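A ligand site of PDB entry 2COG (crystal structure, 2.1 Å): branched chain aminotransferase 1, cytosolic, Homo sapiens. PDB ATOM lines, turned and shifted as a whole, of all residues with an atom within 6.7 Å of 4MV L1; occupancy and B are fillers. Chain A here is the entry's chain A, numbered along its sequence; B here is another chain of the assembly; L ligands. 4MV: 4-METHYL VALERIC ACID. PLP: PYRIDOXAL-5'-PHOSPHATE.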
ATOM      1  N   PHE A  49      -4.116  -1.977 -26.484  1.00  0.00           N
ATOM      2  CA  PHE A  49      -4.919  -1.084 -25.659  1.00  0.00           C
ATOM      3  C   PHE A  49      -4.216  -0.410 -24.478  1.00  0.00           C
ATOM      4  O   PHE A  49      -3.615  -1.073 -23.632  1.00  0.00           O
ATOM      5  CB  PHE A  49      -6.153  -1.824 -25.139  1.00  0.00           C
ATOM      6  CG  PHE A  49      -7.143  -0.935 -24.451  1.00  0.00           C
ATOM      7  CD1 PHE A  49      -8.218  -0.406 -25.159  1.00  0.00           C
ATOM      8  CD2 PHE A  49      -6.990  -0.601 -23.113  1.00  0.00           C
ATOM      9  CE1 PHE A  49      -9.118   0.449 -24.545  1.00  0.00           C
ATOM     10  CE2 PHE A  49      -7.892   0.258 -22.490  1.00  0.00           C
ATOM     11  CZ  PHE A  49      -8.956   0.783 -23.206  1.00  0.00           C
ATOM     12  N   PHE A  95     -12.930   7.170 -12.977  1.00  0.00           N
ATOM     13  CA  PHE A  95     -12.462   7.420 -14.327  1.00  0.00           C
ATOM     14  C   PHE A  95     -13.582   7.373 -15.332  1.00  0.00           C
ATOM     15  O   PHE A  95     -14.739   7.142 -14.985  1.00  0.00           O
ATOM     16  CB  PHE A  95     -11.381   6.396 -14.704  1.00  0.00           C
ATOM     17  CG  PHE A  95     -11.880   4.979 -14.782  1.00  0.00           C
ATOM     18  CD1 PHE A  95     -12.189   4.403 -16.008  1.00  0.00           C
ATOM     19  CD2 PHE A  95     -12.033   4.211 -13.626  1.00  0.00           C
ATOM     20  CE1 PHE A  95     -12.642   3.081 -16.079  1.00  0.00           C
ATOM     21  CE2 PHE A  95     -12.486   2.902 -13.694  1.00  0.00           C
ATOM     22  CZ  PHE A  95     -12.785   2.327 -14.919  1.00  0.00           C
ATOM     23  N   GLY A  97     -14.164   6.774 -19.970  1.00  0.00           N
ATOM     24  CA  GLY A  97     -13.542   6.253 -21.164  1.00  0.00           C
ATOM     25  C   GLY A  97     -14.395   6.497 -22.388  1.00  0.00           C
ATOM     26  O   GLY A  97     -15.472   5.899 -22.528  1.00  0.00           O
ATOM     27  N   LYS A  99     -14.159   7.834 -26.853  1.00  0.00           N
ATOM     28  CA  LYS A  99     -13.281   7.830 -28.017  1.00  0.00           C
ATOM     29  C   LYS A  99     -13.473   8.947 -29.034  1.00  0.00           C
ATOM     30  O   LYS A  99     -14.544   9.553 -29.134  1.00  0.00           O
ATOM     31  CB  LYS A  99     -13.402   6.493 -28.749  1.00  0.00           C
ATOM     32  CG  LYS A  99     -12.880   5.298 -27.985  1.00  0.00           C
ATOM     33  CD  LYS A  99     -12.939   4.047 -28.843  1.00  0.00           C
ATOM     34  CE  LYS A  99     -12.226   2.889 -28.182  1.00  0.00           C
ATOM     35  NZ  LYS A  99     -12.091   1.728 -29.093  1.00  0.00           N
ATOM     36  N   TYR A 161      -8.314   6.607 -27.518  1.00  0.00           N
ATOM     37  CA  TYR A 161      -9.016   6.406 -26.259  1.00  0.00           C
ATOM     38  C   TYR A 161      -8.790   7.592 -25.343  1.00  0.00           C
ATOM     39  O   TYR A 161      -7.655   8.015 -25.141  1.00  0.00           O
ATOM     40  CB  TYR A 161      -8.532   5.115 -25.583  1.00  0.00           C
ATOM     41  CG  TYR A 161      -9.297   4.731 -24.342  1.00  0.00           C
ATOM     42  CD1 TYR A 161     -10.561   4.152 -24.422  1.00  0.00           C
ATOM     43  CD2 TYR A 161      -8.752   4.942 -23.071  1.00  0.00           C
ATOM     44  CE1 TYR A 161     -11.257   3.773 -23.268  1.00  0.00           C
ATOM     45  CE2 TYR A 161      -9.438   4.563 -21.917  1.00  0.00           C
ATOM     46  CZ  TYR A 161     -10.689   3.978 -22.026  1.00  0.00           C
ATOM     47  OH  TYR A 161     -11.344   3.595 -20.877  1.00  0.00           O
ATOM     48  N   ARG A 163      -9.117   8.916 -21.602  1.00  0.00           N
ATOM     49  CA  ARG A 163      -9.241   8.464 -20.220  1.00  0.00           C
ATOM     50  C   ARG A 163      -9.266   9.581 -19.200  1.00  0.00           C
ATOM     51  O   ARG A 163      -8.224   9.992 -18.687  1.00  0.00           O
ATOM     52  CB  ARG A 163      -8.103   7.483 -19.904  1.00  0.00           C
ATOM     53  CG  ARG A 163      -7.929   7.137 -18.420  1.00  0.00           C
ATOM     54  CD  ARG A 163      -9.245   6.692 -17.757  1.00  0.00           C
ATOM     55  NE  ARG A 163      -9.751   5.428 -18.288  1.00  0.00           N
ATOM     56  CZ  ARG A 163      -9.248   4.227 -18.012  1.00  0.00           C
ATOM     57  NH1 ARG A 163      -8.205   4.121 -17.195  1.00  0.00           N
ATOM     58  NH2 ARG A 163      -9.789   3.134 -18.531  1.00  0.00           N
ATOM     59  N   TYR A 193      -9.733  -4.051 -28.051  1.00  0.00           N
ATOM     60  CA  TYR A 193      -9.531  -4.175 -26.601  1.00  0.00           C
ATOM     61  C   TYR A 193      -8.925  -5.523 -26.214  1.00  0.00           C
ATOM     62  O   TYR A 193      -7.928  -5.527 -25.463  1.00  0.00           O
ATOM     63  CB  TYR A 193     -10.870  -3.988 -25.869  1.00  0.00           C
ATOM     64  CG  TYR A 193     -10.780  -3.930 -24.353  1.00  0.00           C
ATOM     65  CD1 TYR A 193      -9.769  -3.193 -23.720  1.00  0.00           C
ATOM     66  CD2 TYR A 193     -11.733  -4.566 -23.557  1.00  0.00           C
ATOM     67  CE1 TYR A 193      -9.717  -3.090 -22.329  1.00  0.00           C
ATOM     68  CE2 TYR A 193     -11.691  -4.464 -22.167  1.00  0.00           C
ATOM     69  CZ  TYR A 193     -10.688  -3.728 -21.557  1.00  0.00           C
ATOM     70  OH  TYR A 193     -10.654  -3.622 -20.182  1.00  0.00           O
ATOM     71  N   LYS A 222     -18.406   4.531 -12.027  1.00  0.00           N
ATOM     72  CA  LYS A 222     -17.105   4.117 -12.536  1.00  0.00           C
ATOM     73  C   LYS A 222     -16.001   4.512 -11.551  1.00  0.00           C
ATOM     74  O   LYS A 222     -15.091   5.264 -11.872  1.00  0.00           O
ATOM     75  CB  LYS A 222     -16.853   4.715 -13.918  1.00  0.00           C
ATOM     76  CG  LYS A 222     -16.682   3.676 -15.013  1.00  0.00           C
ATOM     77  CD  LYS A 222     -16.560   4.307 -16.407  1.00  0.00           C
ATOM     78  CE  LYS A 222     -15.957   3.318 -17.410  1.00  0.00           C
ATOM     79  NZ  LYS A 222     -16.742   2.088 -17.306  1.00  0.00           N
ATOM     80  N   TYR A 227     -12.933  -2.090  -9.334  1.00  0.00           N
ATOM     81  CA  TYR A 227     -12.139  -2.831 -10.296  1.00  0.00           C
ATOM     82  C   TYR A 227     -10.931  -3.562  -9.745  1.00  0.00           C
ATOM     83  O   TYR A 227     -10.593  -4.650 -10.220  1.00  0.00           O
ATOM     84  CB  TYR A 227     -11.701  -1.886 -11.428  1.00  0.00           C
ATOM     85  CG  TYR A 227     -12.886  -1.215 -12.081  1.00  0.00           C
ATOM     86  CD1 TYR A 227     -13.575  -0.188 -11.415  1.00  0.00           C
ATOM     87  CD2 TYR A 227     -13.400  -1.665 -13.301  1.00  0.00           C
ATOM     88  CE1 TYR A 227     -14.730   0.366 -11.948  1.00  0.00           C
ATOM     89  CE2 TYR A 227     -14.574  -1.112 -13.837  1.00  0.00           C
ATOM     90  CZ  TYR A 227     -15.235  -0.109 -13.152  1.00  0.00           C
ATOM     91  OH  TYR A 227     -16.414   0.398 -13.627  1.00  0.00           O
ATOM     92  N   THR A 260     -15.699  -6.085 -17.930  1.00  0.00           N
ATOM     93  CA  THR A 260     -15.968  -4.652 -17.813  1.00  0.00           C
ATOM     94  C   THR A 260     -16.995  -4.185 -18.863  1.00  0.00           C
ATOM     95  O   THR A 260     -16.993  -3.032 -19.249  1.00  0.00           O
ATOM     96  CB  THR A 260     -14.672  -3.812 -17.999  1.00  0.00           C
ATOM     97  OG1 THR A 260     -14.165  -3.982 -19.331  1.00  0.00           O
ATOM     98  CG2 THR A 260     -13.620  -4.229 -16.998  1.00  0.00           C
ATOM     99  N   MET A 261     -17.861  -5.087 -19.312  1.00  0.00           N
ATOM    100  CA  MET A 261     -18.848  -4.742 -20.333  1.00  0.00           C
ATOM    101  C   MET A 261     -20.263  -5.187 -19.973  1.00  0.00           C
ATOM    102  O   MET A 261     -20.446  -6.168 -19.244  1.00  0.00           O
ATOM    103  CB  MET A 261     -18.500  -5.403 -21.663  1.00  0.00           C
ATOM    104  CG  MET A 261     -17.189  -4.964 -22.277  1.00  0.00           C
ATOM    105  SD  MET A 261     -16.861  -5.977 -23.717  1.00  0.00           S
ATOM    106  CE  MET A 261     -16.013  -7.377 -22.945  1.00  0.00           C
ATOM    107  N   ASN A 262     -21.241  -4.464 -20.503  1.00  0.00           N
ATOM    108  CA  ASN A 262     -22.637  -4.814 -20.256  1.00  0.00           C
ATOM    109  C   ASN A 262     -22.958  -6.011 -21.118  1.00  0.00           C
ATOM    110  O   ASN A 262     -22.407  -6.168 -22.208  1.00  0.00           O
ATOM    111  CB  ASN A 262     -23.546  -3.642 -20.587  1.00  0.00           C
ATOM    112  CG  ASN A 262     -23.376  -2.511 -19.610  1.00  0.00           C
ATOM    113  OD1 ASN A 262     -23.678  -2.657 -18.430  1.00  0.00           O
ATOM    114  ND2 ASN A 262     -22.880  -1.373 -20.091  1.00  0.00           N
ATOM    115  N   THR A 290     -22.537   2.488 -24.451  1.00  0.00           N
ATOM    116  CA  THR A 290     -22.809   1.602 -25.572  1.00  0.00           C
ATOM    117  C   THR A 290     -24.112   0.867 -25.344  1.00  0.00           C
ATOM    118  O   THR A 290     -24.861   0.581 -26.280  1.00  0.00           O
ATOM    119  CB  THR A 290     -21.676   0.586 -25.772  1.00  0.00           C
ATOM    120  OG1 THR A 290     -20.407   1.256 -25.757  1.00  0.00           O
ATOM    121  CG2 THR A 290     -21.829  -0.120 -27.113  1.00  0.00           C
ATOM    122  N   SER A 331     -20.856  -5.312 -24.436  1.00  0.00           N
ATOM    123  CA  SER A 331     -20.778  -4.019 -25.093  1.00  0.00           C
ATOM    124  C   SER A 331     -19.979  -3.054 -24.223  1.00  0.00           C
ATOM    125  O   SER A 331     -20.067  -3.122 -22.993  1.00  0.00           O
ATOM    126  CB  SER A 331     -22.188  -3.436 -25.314  1.00  0.00           C
ATOM    127  OG  SER A 331     -22.751  -2.978 -24.088  1.00  0.00           O
ATOM    128  N   GLY A 332     -19.230  -2.164 -24.854  1.00  0.00           N
ATOM    129  CA  GLY A 332     -18.425  -1.205 -24.132  1.00  0.00           C
ATOM    130  C   GLY A 332     -17.633  -0.317 -25.082  1.00  0.00           C
ATOM    131  O   GLY A 332     -17.541  -0.597 -26.271  1.00  0.00           O
ATOM    132  N   THR A 333     -17.059   0.758 -24.573  1.00  0.00           N
ATOM    133  CA  THR A 333     -16.307   1.655 -25.429  1.00  0.00           C
ATOM    134  C   THR A 333     -15.122   0.989 -26.120  1.00  0.00           C
ATOM    135  O   THR A 333     -14.854   1.256 -27.294  1.00  0.00           O
ATOM    136  CB  THR A 333     -15.816   2.877 -24.654  1.00  0.00           C
ATOM    137  OG1 THR A 333     -16.937   3.657 -24.220  1.00  0.00           O
ATOM    138  CG2 THR A 333     -14.900   3.745 -25.531  1.00  0.00           C
ATOM    139  N   ALA A 334     -14.432   0.113 -25.394  1.00  0.00           N
ATOM    140  CA  ALA A 334     -13.262  -0.587 -25.927  1.00  0.00           C
ATOM    141  C   ALA A 334     -13.578  -1.649 -26.973  1.00  0.00           C
ATOM    142  O   ALA A 334     -12.857  -1.779 -27.965  1.00  0.00           O
ATOM    143  CB  ALA A 334     -12.482  -1.210 -24.780  1.00  0.00           C
ATOM    144  N   CYS A 335     -14.645  -2.413 -26.781  1.00  0.00           N
ATOM    145  CA  CYS A 335     -14.980  -3.443 -27.755  1.00  0.00           C
ATOM    146  C   CYS A 335     -16.214  -3.146 -28.614  1.00  0.00           C
ATOM    147  O   CYS A 335     -16.345  -3.676 -29.729  1.00  0.00           O
ATOM    148  CB  CYS A 335     -15.170  -4.795 -27.066  1.00  0.00           C
ATOM    149  SG  CYS A 335     -15.358  -6.123 -28.302  1.00  0.00           S
ATOM    150  N   VAL A 336     -17.112  -2.304 -28.120  1.00  0.00           N
ATOM    151  CA  VAL A 336     -18.342  -1.962 -28.842  1.00  0.00           C
ATOM    152  C   VAL A 336     -19.293  -3.150 -28.795  1.00  0.00           C
ATOM    153  O   VAL A 336     -20.294  -3.130 -28.087  1.00  0.00           O
ATOM    154  CB  VAL A 336     -18.053  -1.613 -30.330  1.00  0.00           C
ATOM    155  CG1 VAL A 336     -19.273  -0.926 -30.938  1.00  0.00           C
ATOM    156  CG2 VAL A 336     -16.805  -0.733 -30.452  1.00  0.00           C
ATOM    157  N   TYR B  90      -7.769   1.695 -11.217  1.00  0.00           N
ATOM    158  CA  TYR B  90      -8.496   0.508 -10.817  1.00  0.00           C
ATOM    159  C   TYR B  90      -8.314   0.064  -9.380  1.00  0.00           C
ATOM    160  O   TYR B  90      -8.540  -1.097  -9.063  1.00  0.00           O
ATOM    161  CB  TYR B  90      -8.126  -0.647 -11.761  1.00  0.00           C
ATOM    162  CG  TYR B  90      -8.203  -0.244 -13.220  1.00  0.00           C
ATOM    163  CD1 TYR B  90      -7.070  -0.287 -14.038  1.00  0.00           C
ATOM    164  CD2 TYR B  90      -9.386   0.242 -13.752  1.00  0.00           C
ATOM    165  CE1 TYR B  90      -7.132   0.147 -15.362  1.00  0.00           C
ATOM    166  CE2 TYR B  90      -9.460   0.681 -15.069  1.00  0.00           C
ATOM    167  CZ  TYR B  90      -8.328   0.634 -15.873  1.00  0.00           C
ATOM    168  OH  TYR B  90      -8.404   1.111 -17.165  1.00  0.00           O
ATOM    169  N   LEU B 173      -3.378   1.076 -19.514  1.00  0.00           N
ATOM    170  CA  LEU B 173      -4.744   1.238 -19.003  1.00  0.00           C
ATOM    171  C   LEU B 173      -5.568  -0.045 -18.990  1.00  0.00           C
ATOM    172  O   LEU B 173      -6.728  -0.029 -18.579  1.00  0.00           O
ATOM    173  CB  LEU B 173      -5.469   2.309 -19.813  1.00  0.00           C
ATOM    174  CG  LEU B 173      -4.699   3.625 -19.992  1.00  0.00           C
ATOM    175  CD1 LEU B 173      -5.487   4.597 -20.856  1.00  0.00           C
ATOM    176  CD2 LEU B 173      -4.416   4.228 -18.622  1.00  0.00           C
ATOM    177  N   GLY B 174      -5.002  -1.153 -19.426  1.00  0.00           N
ATOM    178  CA  GLY B 174      -5.767  -2.389 -19.409  1.00  0.00           C
ATOM    179  C   GLY B 174      -6.007  -2.845 -17.981  1.00  0.00           C
ATOM    180  O   GLY B 174      -5.146  -2.701 -17.123  1.00  0.00           O
ATOM    181  N   VAL B 175      -7.188  -3.400 -17.716  1.00  0.00           N
ATOM    182  CA  VAL B 175      -7.499  -3.889 -16.369  1.00  0.00           C
ATOM    183  C   VAL B 175      -6.948  -5.299 -16.210  1.00  0.00           C
ATOM    184  O   VAL B 175      -7.575  -6.265 -16.615  1.00  0.00           O
ATOM    185  CB  VAL B 175      -9.034  -3.926 -16.112  1.00  0.00           C
ATOM    186  CG1 VAL B 175      -9.319  -4.609 -14.778  1.00  0.00           C
ATOM    187  CG2 VAL B 175      -9.602  -2.524 -16.106  1.00  0.00           C
HETATM  188  CA  4MV L   1     -14.118  -0.255 -20.465  1.00  0.00           C
HETATM  189  CB  4MV L   1     -12.606  -0.533 -20.330  1.00  0.00           C
HETATM  190  CG  4MV L   1     -11.961   0.039 -19.049  1.00  0.00           C
HETATM  191  CD1 4MV L   1     -12.639  -0.563 -17.821  1.00  0.00           C
HETATM  192  CD2 4MV L   1     -10.476  -0.274 -19.037  1.00  0.00           C
HETATM  193  C   4MV L   1     -14.725  -0.822 -21.732  1.00  0.00           C
HETATM  194  O   4MV L   1     -14.724  -0.102 -22.761  1.00  0.00           O
HETATM  195  OXT 4MV L   1     -15.212  -1.981 -21.705  1.00  0.00           O
HETATM  196  N1  PLP L   2     -19.417  -2.105 -17.275  1.00  0.00           N
HETATM  197  C2  PLP L   2     -18.429  -1.660 -16.450  1.00  0.00           C
HETATM  198  C2A PLP L   2     -18.203  -2.367 -15.086  1.00  0.00           C
HETATM  199  C3  PLP L   2     -17.672  -0.578 -16.831  1.00  0.00           C
HETATM  200  O3  PLP L   2     -16.662  -0.120 -16.022  1.00  0.00           O
HETATM  201  C4  PLP L   2     -17.902   0.045 -18.041  1.00  0.00           C
HETATM  202  C4A PLP L   2     -17.021   1.262 -18.381  1.00  0.00           C
HETATM  203  C5  PLP L   2     -18.928  -0.450 -18.876  1.00  0.00           C
HETATM  204  C6  PLP L   2     -19.659  -1.516 -18.465  1.00  0.00           C
HETATM  205  C5A PLP L   2     -19.258   0.119 -20.264  1.00  0.00           C
HETATM  206  O4P PLP L   2     -19.700   1.447 -20.397  1.00  0.00           O
HETATM  207  P   PLP L   2     -19.436   2.159 -21.822  1.00  0.00           P
HETATM  208  O1P PLP L   2     -17.991   2.135 -22.170  1.00  0.00           O
HETATM  209  O2P PLP L   2     -19.867   3.610 -21.327  1.00  0.00           O
HETATM  210  O3P PLP L   2     -20.427   1.619 -22.790  1.00  0.00           O
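The backbone NH (N) of Ala 334 lies close to an oxygen (O) of 4MV L1 (2.7 Å). An oxygen (O) of 4MV L1 lies close to the backbone NH (N) of Thr 333 (3.1 Å). OXT of 4MV L1 lies close to O of Thr 260 (3.2 Å). OG1 of Thr 260 lies close to OXT of 4MV L1 (3.3 Å). The backbone NH (N) of Thr 333 lies close to an oxygen (O1P) of PLP L2, 2.9 Å away. O1P of PLP L2 lies close to OG1 of Thr 333 (2.8 Å). The backbone carbonyl oxygen (O) of Thr 260 lies close to a nitrogen (N1) of PLP L2. An oxygen (O3) of PLP L2 lies close to the side-chain hydroxyl (OH) of Tyr 227 (2.5 Å). C4A of PLP L2 is bonded to NZ of Lys 222 (1.4 Å). O3P of PLP L2 lies close to N of Thr 290. The side-chain hydroxyl of Thr 290 lies close to an oxygen (O3P) of PLP L2 (3.0 Å).
The backbone carbonyl oxygen (O) of Gly 97 is in hydrogen-bond range of the side-chain hydroxyl (OG1) of Thr 333 (3.2 Å). The backbone carbonyl oxygen (O) of Thr 333 lies close to the side-chain amino group (NZ) of Lys 99 (3.3 Å). NH2 of Arg 163 sits at hydrogen-bond distance from OH of Tyr 90 of chain B. OH of Tyr 90 of chain B is in hydrogen-bond range of O of Leu 173 of chain B, at 2.5 Å. The guanidinium group (NH2) of Arg 163 sits at hydrogen-bond distance from the side-chain hydroxyl (OH) of Tyr 161, 2.9 Å away. O of Gly 332 lies close to OG1 of Thr 290 (3.5 Å).
Merely in contact with 4MV L1: Arg 163 (3.5 Å), Tyr 193 (3.5 Å), Met 261 (3.6 Å), Gly 332 (3.7 Å), Tyr 90 of chain B (3.1 Å), Leu 173 of chain B (3.8 Å) and Val 175 of chain B (3.8 Å). Hydrophobic or aromatic side chains within 4 Å of 4MV L1: Tyr 193, Met 261, Ala 334, Tyr 90 of chain B and Val 175 of chain B.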
